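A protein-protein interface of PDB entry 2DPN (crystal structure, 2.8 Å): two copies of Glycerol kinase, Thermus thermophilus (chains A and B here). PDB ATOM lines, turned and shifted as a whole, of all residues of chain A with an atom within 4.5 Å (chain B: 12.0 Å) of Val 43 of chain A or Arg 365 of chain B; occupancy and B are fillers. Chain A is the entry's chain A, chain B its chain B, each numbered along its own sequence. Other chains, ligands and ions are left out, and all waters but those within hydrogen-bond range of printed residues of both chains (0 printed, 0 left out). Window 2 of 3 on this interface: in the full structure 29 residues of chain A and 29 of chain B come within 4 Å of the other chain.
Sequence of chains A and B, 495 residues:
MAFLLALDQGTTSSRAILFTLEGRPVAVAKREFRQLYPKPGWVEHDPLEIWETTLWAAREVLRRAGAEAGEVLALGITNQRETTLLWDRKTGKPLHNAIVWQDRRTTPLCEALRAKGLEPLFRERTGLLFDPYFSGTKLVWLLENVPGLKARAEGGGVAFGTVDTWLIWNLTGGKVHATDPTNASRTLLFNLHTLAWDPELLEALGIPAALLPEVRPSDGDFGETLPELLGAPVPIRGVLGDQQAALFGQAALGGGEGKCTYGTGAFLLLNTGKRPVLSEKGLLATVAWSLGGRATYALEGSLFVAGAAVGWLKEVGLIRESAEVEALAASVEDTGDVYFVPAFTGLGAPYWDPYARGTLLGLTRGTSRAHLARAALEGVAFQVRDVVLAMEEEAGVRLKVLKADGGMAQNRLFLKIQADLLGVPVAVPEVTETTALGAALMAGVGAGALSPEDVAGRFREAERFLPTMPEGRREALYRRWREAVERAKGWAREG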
ATOM      1  N   LEU A  36      37.748 -25.468  20.494  1.00  0.00           N
ATOM      2  CA  LEU A  36      37.394 -25.730  19.106  1.00  0.00           C
ATOM      3  C   LEU A  36      36.006 -26.319  18.925  1.00  0.00           C
ATOM      4  O   LEU A  36      35.653 -27.307  19.562  1.00  0.00           O
ATOM      5  CB  LEU A  36      38.450 -26.637  18.469  1.00  0.00           C
ATOM      6  CG  LEU A  36      39.863 -26.049  18.519  1.00  0.00           C
ATOM      7  CD1 LEU A  36      40.847 -27.028  17.942  1.00  0.00           C
ATOM      8  CD2 LEU A  36      39.902 -24.740  17.756  1.00  0.00           C
ATOM      9  N   TYR A  37      35.227 -25.702  18.038  1.00  0.00           N
ATOM     10  CA  TYR A  37      33.852 -26.123  17.742  1.00  0.00           C
ATOM     11  C   TYR A  37      33.687 -26.429  16.252  1.00  0.00           C
ATOM     12  O   TYR A  37      33.125 -25.629  15.516  1.00  0.00           O
ATOM     13  CB  TYR A  37      32.895 -25.007  18.141  1.00  0.00           C
ATOM     14  CG  TYR A  37      33.035 -24.587  19.586  1.00  0.00           C
ATOM     15  CD1 TYR A  37      32.824 -25.494  20.616  1.00  0.00           C
ATOM     16  CD2 TYR A  37      33.356 -23.278  19.923  1.00  0.00           C
ATOM     17  CE1 TYR A  37      32.920 -25.115  21.940  1.00  0.00           C
ATOM     18  CE2 TYR A  37      33.458 -22.882  21.252  1.00  0.00           C
ATOM     19  CZ  TYR A  37      33.236 -23.806  22.258  1.00  0.00           C
ATOM     20  OH  TYR A  37      33.315 -23.421  23.582  1.00  0.00           O
ATOM     21  N   GLY A  41      27.647 -28.623  18.467  1.00  0.00           N
ATOM     22  CA  GLY A  41      27.588 -29.679  19.461  1.00  0.00           C
ATOM     23  C   GLY A  41      28.906 -30.432  19.568  1.00  0.00           C
ATOM     24  O   GLY A  41      29.062 -31.320  20.397  1.00  0.00           O
ATOM     25  N   TRP A  42      29.853 -30.095  18.704  1.00  0.00           N
ATOM     26  CA  TRP A  42      31.157 -30.726  18.723  1.00  0.00           C
ATOM     27  C   TRP A  42      32.123 -29.826  19.502  1.00  0.00           C
ATOM     28  O   TRP A  42      32.103 -28.600  19.355  1.00  0.00           O
ATOM     29  CB  TRP A  42      31.644 -30.931  17.290  1.00  0.00           C
ATOM     30  CG  TRP A  42      30.981 -32.092  16.606  1.00  0.00           C
ATOM     31  CD1 TRP A  42      29.714 -32.562  16.823  1.00  0.00           C
ATOM     32  CD2 TRP A  42      31.545 -32.920  15.581  1.00  0.00           C
ATOM     33  NE1 TRP A  42      29.464 -33.628  15.996  1.00  0.00           N
ATOM     34  CE2 TRP A  42      30.572 -33.865  15.225  1.00  0.00           C
ATOM     35  CE3 TRP A  42      32.780 -32.947  14.928  1.00  0.00           C
ATOM     36  CZ2 TRP A  42      30.796 -34.829  14.251  1.00  0.00           C
ATOM     37  CZ3 TRP A  42      33.002 -33.907  13.957  1.00  0.00           C
ATOM     38  CH2 TRP A  42      32.015 -34.832  13.629  1.00  0.00           C
ATOM     39  N   VAL A  43      32.953 -30.436  20.342  1.00  0.00           N
ATOM     40  CA  VAL A  43      33.905 -29.687  21.166  1.00  0.00           C
ATOM     41  C   VAL A  43      35.296 -30.329  21.170  1.00  0.00           C
ATOM     42  O   VAL A  43      35.450 -31.476  21.588  1.00  0.00           O
ATOM     43  CB  VAL A  43      33.397 -29.597  22.624  1.00  0.00           C
ATOM     44  CG1 VAL A  43      34.385 -28.816  23.479  1.00  0.00           C
ATOM     45  CG2 VAL A  43      32.043 -28.945  22.654  1.00  0.00           C
ATOM     46  N   GLU A  44      36.306 -29.597  20.715  1.00  0.00           N
ATOM     47  CA  GLU A  44      37.643 -30.197  20.714  1.00  0.00           C
ATOM     48  C   GLU A  44      38.704 -29.281  21.349  1.00  0.00           C
ATOM     49  O   GLU A  44      38.501 -28.088  21.531  1.00  0.00           O
ATOM     50  CB  GLU A  44      38.024 -30.511  19.267  1.00  0.00           C
ATOM     51  CG  GLU A  44      36.952 -31.326  18.545  1.00  0.00           C
ATOM     52  CD  GLU A  44      37.548 -31.954  17.307  1.00  0.00           C
ATOM     53  OE1 GLU A  44      38.103 -31.231  16.491  1.00  0.00           O
ATOM     54  OE2 GLU A  44      37.448 -33.172  17.164  1.00  0.00           O
ATOM     55  N   ALA A  98      41.842 -33.607  20.851  1.00  0.00           N
ATOM     56  CA  ALA A  98      41.180 -34.264  21.967  1.00  0.00           C
ATOM     57  C   ALA A  98      39.681 -33.977  21.950  1.00  0.00           C
ATOM     58  O   ALA A  98      39.252 -32.825  21.847  1.00  0.00           O
ATOM     59  CB  ALA A  98      41.780 -33.795  23.272  1.00  0.00           C
ATOM     60  N   ILE A  99      38.877 -35.026  22.038  1.00  0.00           N
ATOM     61  CA  ILE A  99      37.440 -34.829  22.052  1.00  0.00           C
ATOM     62  C   ILE A  99      37.045 -34.593  23.503  1.00  0.00           C
ATOM     63  O   ILE A  99      37.085 -35.490  24.336  1.00  0.00           O
ATOM     64  CB  ILE A  99      36.691 -36.038  21.410  1.00  0.00           C
ATOM     65  CG1 ILE A  99      37.054 -36.096  19.924  1.00  0.00           C
ATOM     66  CG2 ILE A  99      35.177 -35.876  21.529  1.00  0.00           C
ATOM     67  CD1 ILE A  99      36.437 -37.237  19.158  1.00  0.00           C
ATOM     68  N   VAL A 100      36.700 -33.343  23.782  1.00  0.00           N
ATOM     69  CA  VAL A 100      36.306 -32.883  25.105  1.00  0.00           C
ATOM     70  C   VAL A 100      35.021 -33.546  25.620  1.00  0.00           C
ATOM     71  O   VAL A 100      34.218 -34.059  24.847  1.00  0.00           O
ATOM     72  CB  VAL A 100      36.131 -31.337  25.083  1.00  0.00           C
ATOM     73  CG1 VAL A 100      36.023 -30.798  26.486  1.00  0.00           C
ATOM     74  CG2 VAL A 100      37.305 -30.690  24.353  1.00  0.00           C
ATOM     75  N   GLN A 102      32.437 -32.237  26.671  1.00  0.00           N
ATOM     76  CA  GLN A 102      31.245 -31.518  26.271  1.00  0.00           C
ATOM     77  C   GLN A 102      30.746 -31.997  24.924  1.00  0.00           C
ATOM     78  O   GLN A 102      29.565 -31.887  24.614  1.00  0.00           O
ATOM     79  CB  GLN A 102      31.538 -30.017  26.196  1.00  0.00           C
ATOM     80  CG  GLN A 102      32.250 -29.474  27.422  1.00  0.00           C
ATOM     81  CD  GLN A 102      32.438 -27.967  27.391  1.00  0.00           C
ATOM     82  OE1 GLN A 102      33.118 -27.423  26.514  1.00  0.00           O
ATOM     83  NE2 GLN A 102      31.832 -27.284  28.357  1.00  0.00           N
ATOM     84  N   ASP A 103      31.650 -32.539  24.121  1.00  0.00           N
ATOM     85  CA  ASP A 103      31.292 -32.983  22.788  1.00  0.00           C
ATOM     86  C   ASP A 103      30.097 -33.919  22.804  1.00  0.00           C
ATOM     87  O   ASP A 103      29.811 -34.548  23.817  1.00  0.00           O
ATOM     88  CB  ASP A 103      32.490 -33.644  22.110  1.00  0.00           C
ATOM     89  CG  ASP A 103      32.238 -33.911  20.650  1.00  0.00           C
ATOM     90  OD1 ASP A 103      31.545 -34.899  20.344  1.00  0.00           O
ATOM     91  OD2 ASP A 103      32.702 -33.120  19.804  1.00  0.00           O
ATOM     92  N   ALA A 308      28.396 -21.350  31.625  1.00  0.00           N
ATOM     93  CA  ALA A 308      27.995 -21.047  30.264  1.00  0.00           C
ATOM     94  C   ALA A 308      26.611 -20.431  30.159  1.00  0.00           C
ATOM     95  O   ALA A 308      26.328 -19.730  29.197  1.00  0.00           O
ATOM     96  CB  ALA A 308      28.053 -22.295  29.428  1.00  0.00           C
ATOM     97  N   TRP A 312      26.696 -17.481  27.845  1.00  0.00           N
ATOM     98  CA  TRP A 312      25.847 -17.352  26.672  1.00  0.00           C
ATOM     99  C   TRP A 312      25.163 -15.985  26.664  1.00  0.00           C
ATOM    100  O   TRP A 312      25.140 -15.293  25.646  1.00  0.00           O
ATOM    101  CB  TRP A 312      24.802 -18.471  26.647  1.00  0.00           C
ATOM    102  CG  TRP A 312      23.906 -18.356  25.471  1.00  0.00           C
ATOM    103  CD1 TRP A 312      24.232 -18.593  24.168  1.00  0.00           C
ATOM    104  CD2 TRP A 312      22.567 -17.851  25.465  1.00  0.00           C
ATOM    105  NE1 TRP A 312      23.185 -18.257  23.347  1.00  0.00           N
ATOM    106  CE2 TRP A 312      22.147 -17.800  24.118  1.00  0.00           C
ATOM    107  CE3 TRP A 312      21.685 -17.430  26.464  1.00  0.00           C
ATOM    108  CZ2 TRP A 312      20.874 -17.342  23.745  1.00  0.00           C
ATOM    109  CZ3 TRP A 312      20.425 -16.974  26.094  1.00  0.00           C
ATOM    110  CH2 TRP A 312      20.031 -16.935  24.746  1.00  0.00           C
ATOM    111  N   GLU A 315      27.552 -13.715  25.379  1.00  0.00           N
ATOM    112  CA  GLU A 315      27.714 -13.806  23.931  1.00  0.00           C
ATOM    113  C   GLU A 315      26.597 -13.122  23.161  1.00  0.00           C
ATOM    114  O   GLU A 315      26.866 -12.380  22.224  1.00  0.00           O
ATOM    115  CB  GLU A 315      27.839 -15.274  23.483  1.00  0.00           C
ATOM    116  CG  GLU A 315      29.198 -15.912  23.829  1.00  0.00           C
ATOM    117  CD  GLU A 315      29.381 -17.347  23.304  1.00  0.00           C
ATOM    118  OE1 GLU A 315      28.666 -18.267  23.770  1.00  0.00           O
ATOM    119  OE2 GLU A 315      30.251 -17.558  22.423  1.00  0.00           O
ATOM    120  N   PHE A 344      21.825 -26.276  26.504  1.00  0.00           N
ATOM    121  CA  PHE A 344      22.293 -26.179  25.123  1.00  0.00           C
ATOM    122  C   PHE A 344      22.704 -27.502  24.465  1.00  0.00           C
ATOM    123  O   PHE A 344      22.378 -27.748  23.306  1.00  0.00           O
ATOM    124  CB  PHE A 344      23.470 -25.205  25.026  1.00  0.00           C
ATOM    125  CG  PHE A 344      23.244 -23.901  25.732  1.00  0.00           C
ATOM    126  CD1 PHE A 344      22.025 -23.230  25.624  1.00  0.00           C
ATOM    127  CD2 PHE A 344      24.257 -23.332  26.499  1.00  0.00           C
ATOM    128  CE1 PHE A 344      21.819 -22.008  26.274  1.00  0.00           C
ATOM    129  CE2 PHE A 344      24.058 -22.109  27.152  1.00  0.00           C
ATOM    130  CZ  PHE A 344      22.837 -21.448  27.038  1.00  0.00           C
ATOM    131  N   THR A 345      23.414 -28.354  25.204  1.00  0.00           N
ATOM    132  CA  THR A 345      23.881 -29.617  24.637  1.00  0.00           C
ATOM    133  C   THR A 345      23.149 -30.825  25.231  1.00  0.00           C
ATOM    134  O   THR A 345      23.653 -31.941  25.270  1.00  0.00           O
ATOM    135  CB  THR A 345      25.377 -29.740  24.920  1.00  0.00           C
ATOM    136  OG1 THR A 345      25.590 -29.648  26.330  1.00  0.00           O
ATOM    137  CG2 THR A 345      26.133 -28.603  24.229  1.00  0.00           C
ATOM    138  N   THR B 335      18.202 -20.173  11.627  1.00  0.00           N
ATOM    139  CA  THR B 335      18.232 -19.769  13.025  1.00  0.00           C
ATOM    140  C   THR B 335      18.933 -20.802  13.896  1.00  0.00           C
ATOM    141  O   THR B 335      19.000 -20.649  15.112  1.00  0.00           O
ATOM    142  CB  THR B 335      16.828 -19.584  13.571  1.00  0.00           C
ATOM    143  OG1 THR B 335      16.190 -20.860  13.640  1.00  0.00           O
ATOM    144  CG2 THR B 335      16.026 -18.679  12.673  1.00  0.00           C
ATOM    145  N   GLY B 336      19.444 -21.856  13.269  1.00  0.00           N
ATOM    146  CA  GLY B 336      20.134 -22.906  13.998  1.00  0.00           C
ATOM    147  C   GLY B 336      19.195 -23.876  14.690  1.00  0.00           C
ATOM    148  O   GLY B 336      19.605 -24.615  15.586  1.00  0.00           O
ATOM    149  N   ASP B 337      17.938 -23.871  14.252  1.00  0.00           N
ATOM    150  CA  ASP B 337      16.864 -24.704  14.789  1.00  0.00           C
ATOM    151  C   ASP B 337      16.267 -24.041  16.014  1.00  0.00           C
ATOM    152  O   ASP B 337      15.757 -24.701  16.920  1.00  0.00           O
ATOM    153  CB  ASP B 337      17.337 -26.132  15.106  1.00  0.00           C
ATOM    154  CG  ASP B 337      16.168 -27.091  15.377  1.00  0.00           C
ATOM    155  OD1 ASP B 337      15.143 -26.985  14.675  1.00  0.00           O
ATOM    156  OD2 ASP B 337      16.265 -27.956  16.271  1.00  0.00           O
ATOM    157  N   VAL B 338      16.352 -22.718  16.037  1.00  0.00           N
ATOM    158  CA  VAL B 338      15.793 -21.941  17.130  1.00  0.00           C
ATOM    159  C   VAL B 338      14.412 -21.431  16.719  1.00  0.00           C
ATOM    160  O   VAL B 338      14.177 -21.095  15.556  1.00  0.00           O
ATOM    161  CB  VAL B 338      16.699 -20.749  17.497  1.00  0.00           C
ATOM    162  CG1 VAL B 338      16.040 -19.914  18.569  1.00  0.00           C
ATOM    163  CG2 VAL B 338      18.017 -21.254  18.014  1.00  0.00           C
ATOM    164  N   LEU B 361      13.131 -21.701  21.809  1.00  0.00           N
ATOM    165  CA  LEU B 361      13.439 -23.120  21.767  1.00  0.00           C
ATOM    166  C   LEU B 361      14.667 -23.483  20.949  1.00  0.00           C
ATOM    167  O   LEU B 361      14.984 -22.826  19.960  1.00  0.00           O
ATOM    168  CB  LEU B 361      12.232 -23.885  21.225  1.00  0.00           C
ATOM    169  CG  LEU B 361      10.980 -23.815  22.093  1.00  0.00           C
ATOM    170  CD1 LEU B 361       9.806 -24.415  21.340  1.00  0.00           C
ATOM    171  CD2 LEU B 361      11.223 -24.555  23.413  1.00  0.00           C
ATOM    172  N   GLY B 362      15.352 -24.536  21.387  1.00  0.00           N
ATOM    173  CA  GLY B 362      16.517 -25.031  20.684  1.00  0.00           C
ATOM    174  C   GLY B 362      17.782 -24.218  20.788  1.00  0.00           C
ATOM    175  O   GLY B 362      18.606 -24.248  19.874  1.00  0.00           O
ATOM    176  N   LEU B 363      17.948 -23.495  21.889  1.00  0.00           N
ATOM    177  CA  LEU B 363      19.151 -22.695  22.081  1.00  0.00           C
ATOM    178  C   LEU B 363      20.329 -23.626  22.331  1.00  0.00           C
ATOM    179  O   LEU B 363      20.199 -24.641  23.006  1.00  0.00           O
ATOM    180  CB  LEU B 363      18.984 -21.753  23.269  1.00  0.00           C
ATOM    181  CG  LEU B 363      17.795 -20.791  23.228  1.00  0.00           C
ATOM    182  CD1 LEU B 363      17.640 -20.174  24.612  1.00  0.00           C
ATOM    183  CD2 LEU B 363      17.990 -19.712  22.149  1.00  0.00           C
ATOM    184  N   THR B 364      21.477 -23.274  21.773  1.00  0.00           N
ATOM    185  CA  THR B 364      22.690 -24.066  21.926  1.00  0.00           C
ATOM    186  C   THR B 364      23.845 -23.112  22.189  1.00  0.00           C
ATOM    187  O   THR B 364      23.719 -21.911  21.968  1.00  0.00           O
ATOM    188  CB  THR B 364      22.967 -24.851  20.663  1.00  0.00           C
ATOM    189  OG1 THR B 364      23.026 -23.948  19.556  1.00  0.00           O
ATOM    190  CG2 THR B 364      21.858 -25.842  20.414  1.00  0.00           C
ATOM    191  N   ARG B 365      24.970 -23.633  22.658  1.00  0.00           N
ATOM    192  CA  ARG B 365      26.115 -22.785  22.981  1.00  0.00           C
ATOM    193  C   ARG B 365      26.412 -21.774  21.863  1.00  0.00           C
ATOM    194  O   ARG B 365      27.025 -20.732  22.070  1.00  0.00           O
ATOM    195  CB  ARG B 365      27.318 -23.705  23.225  1.00  0.00           C
ATOM    196  CG  ARG B 365      28.666 -22.975  23.160  1.00  0.00           C
ATOM    197  CD  ARG B 365      29.682 -23.536  24.166  1.00  0.00           C
ATOM    198  NE  ARG B 365      29.828 -24.987  24.025  1.00  0.00           N
ATOM    199  CZ  ARG B 365      29.649 -25.727  25.135  1.00  0.00           C
ATOM    200  NH1 ARG B 365      29.357 -25.139  26.282  1.00  0.00           N
ATOM    201  NH2 ARG B 365      29.739 -27.060  25.067  1.00  0.00           N
ATOM    202  N   GLY B 366      25.960 -22.126  20.642  1.00  0.00           N
ATOM    203  CA  GLY B 366      26.288 -21.304  19.482  1.00  0.00           C
ATOM    204  C   GLY B 366      25.132 -20.407  19.021  1.00  0.00           C
ATOM    205  O   GLY B 366      25.266 -19.618  18.092  1.00  0.00           O
ATOM    206  N   THR B 367      23.955 -20.567  19.653  1.00  0.00           N
ATOM    207  CA  THR B 367      22.888 -19.623  19.333  1.00  0.00           C
ATOM    208  C   THR B 367      23.372 -18.181  19.520  1.00  0.00           C
ATOM    209  O   THR B 367      23.970 -17.816  20.525  1.00  0.00           O
ATOM    210  CB  THR B 367      21.685 -19.893  20.241  1.00  0.00           C
ATOM    211  OG1 THR B 367      21.234 -21.234  20.047  1.00  0.00           O
ATOM    212  CG2 THR B 367      20.548 -18.937  19.882  1.00  0.00           C
ATOM    213  N   SER B 368      23.134 -17.358  18.488  1.00  0.00           N
ATOM    214  CA  SER B 368      23.622 -15.985  18.568  1.00  0.00           C
ATOM    215  C   SER B 368      22.504 -14.963  18.365  1.00  0.00           C
ATOM    216  O   SER B 368      21.336 -15.304  18.233  1.00  0.00           O
ATOM    217  CB  SER B 368      24.695 -15.797  17.500  1.00  0.00           C
ATOM    218  OG  SER B 368      24.074 -15.430  16.267  1.00  0.00           O
ATOM    219  N   ARG B 369      22.899 -13.693  18.324  1.00  0.00           N
ATOM    220  CA  ARG B 369      21.969 -12.585  18.149  1.00  0.00           C
ATOM    221  C   ARG B 369      21.339 -12.571  16.772  1.00  0.00           C
ATOM    222  O   ARG B 369      20.156 -12.246  16.618  1.00  0.00           O
ATOM    223  CB  ARG B 369      22.685 -11.265  18.382  1.00  0.00           C
ATOM    224  CG  ARG B 369      23.077 -11.036  19.819  1.00  0.00           C
ATOM    225  CD  ARG B 369      23.969  -9.814  19.936  1.00  0.00           C
ATOM    226  NE  ARG B 369      23.496  -8.735  19.078  1.00  0.00           N
ATOM    227  CZ  ARG B 369      23.992  -7.505  19.088  1.00  0.00           C
ATOM    228  NH1 ARG B 369      24.981  -7.199  19.929  1.00  0.00           N
ATOM    229  NH2 ARG B 369      23.514  -6.592  18.243  1.00  0.00           N
ATOM    230  N   ALA B 370      22.142 -12.897  15.766  1.00  0.00           N
ATOM    231  CA  ALA B 370      21.633 -12.938  14.404  1.00  0.00           C
ATOM    232  C   ALA B 370      20.491 -13.959  14.390  1.00  0.00           C
ATOM    233  O   ALA B 370      19.397 -13.699  13.879  1.00  0.00           O
ATOM    234  CB  ALA B 370      22.739 -13.367  13.451  1.00  0.00           C
ATOM    235  N   HIS B 371      20.768 -15.111  14.990  1.00  0.00           N
ATOM    236  CA  HIS B 371      19.820 -16.204  15.087  1.00  0.00           C
ATOM    237  C   HIS B 371      18.526 -15.832  15.811  1.00  0.00           C
ATOM    238  O   HIS B 371      17.439 -16.173  15.358  1.00  0.00           O
ATOM    239  CB  HIS B 371      20.497 -17.383  15.780  1.00  0.00           C
ATOM    240  CG  HIS B 371      21.518 -18.071  14.930  1.00  0.00           C
ATOM    241  ND1 HIS B 371      22.718 -18.530  15.429  1.00  0.00           N
ATOM    242  CD2 HIS B 371      21.506 -18.401  13.618  1.00  0.00           C
ATOM    243  CE1 HIS B 371      23.403 -19.112  14.460  1.00  0.00           C
ATOM    244  NE2 HIS B 371      22.689 -19.048  13.351  1.00  0.00           N
ATOM    245  N   LEU B 372      18.644 -15.138  16.937  1.00  0.00           N
ATOM    246  CA  LEU B 372      17.471 -14.733  17.708  1.00  0.00           C
ATOM    247  C   LEU B 372      16.657 -13.707  16.934  1.00  0.00           C
ATOM    248  O   LEU B 372      15.429 -13.668  17.023  1.00  0.00           O
ATOM    249  CB  LEU B 372      17.904 -14.135  19.049  1.00  0.00           C
ATOM    250  CG  LEU B 372      18.645 -15.083  19.990  1.00  0.00           C
ATOM    251  CD1 LEU B 372      19.052 -14.344  21.256  1.00  0.00           C
ATOM    252  CD2 LEU B 372      17.738 -16.267  20.319  1.00  0.00           C
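The indole nitrogen (NE1) of Trp 312 of chain A is in hydrogen-bond range of the backbone carbonyl oxygen (O) of Thr 367 of chain B (3.0 Å). The side-chain carboxylate of Glu 315 of chain A sits close to the backbone carbonyl oxygen of Arg 365 of chain B, 3.4 Å away.
OG1 of Thr 367 of chain B sits at hydrogen-bond distance from N of Thr 364 of chain B (2.7 Å). The backbone NH (N) of Val 43 of chain A is in hydrogen-bond range of the side-chain carboxylate (OD2) of Asp 103 of chain A. The backbone NH of Val 100 of chain A lies within hydrogen-bond range of the backbone carbonyl oxygen of Val 43 of chain A.
Among the printed residues, merely in contact across the chains: Tyr 37 of chain A with Arg 365 of chain B (3.7 Å), Val 43 of chain A with Arg 365 of chain B (3.8 Å), Gln 102 of chain A with Arg 365 of chain B (3.6 Å), Trp 312 of chain A with Thr 364 of chain B (3.9 Å), Phe 344 of chain A with Leu 363 of chain B (3.4 Å), Phe 344 of chain A with Thr 364 of chain B (3.4 Å) and Phe 344 of chain A with Arg 365 of chain B (3.2 Å).
Of the printed residues of chain A, Arg 365 of chain B touches Tyr 37 (3.7 Å), Val 43 (3.8 Å), Gln 102 (3.6 Å), Glu 315 (3.4 Å) and Phe 344 (3.2 Å). Gly 41 of chain A touches none of the printed residues of chain B. No residue of chain B comes within 4 Å of Glu 44 of chain A. No residue of chain B comes within 4 Å of Ala 98 of chain A. No residue of chain B comes within 4 Å of Ile 99 of chain A. No residue of chain B comes within 4 Å of Asp 103 of chain A. Ala 308 of chain A touches none of the printed residues of chain B. Printed residues of chain A within 4 Å of Thr 367 of chain B: Trp 312. Printed residues of chain A within 4 Å of Thr 364 of chain B: Trp 312 and Phe 344. The nearest residue of chain B that does not touch Val 43 of chain A is Gly 366 of chain B (9.4 Å). The nearest printed residue of chain A that does not touch Arg 365 of chain B is Thr 345 of chain A (4.01 Å). The nearest printed residue of chain A that does not touch Leu 363 of chain B is Trp 312 of chain A (4.03 Å).
Hydrophobic or aromatic side chains of chain A that line the printed part of chain B: Tyr 37, Val 43, Trp 312 and Phe 344. Among the printed residues, no Asp or Glu carboxylate lies within 4 Å of a Lys or Arg side-chain nitrogen of the other chain.
No position is printed for both chains. Of the 9 pairs that touch across the chains among the printed residues, none has its exchanged pair printed and touching as well.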
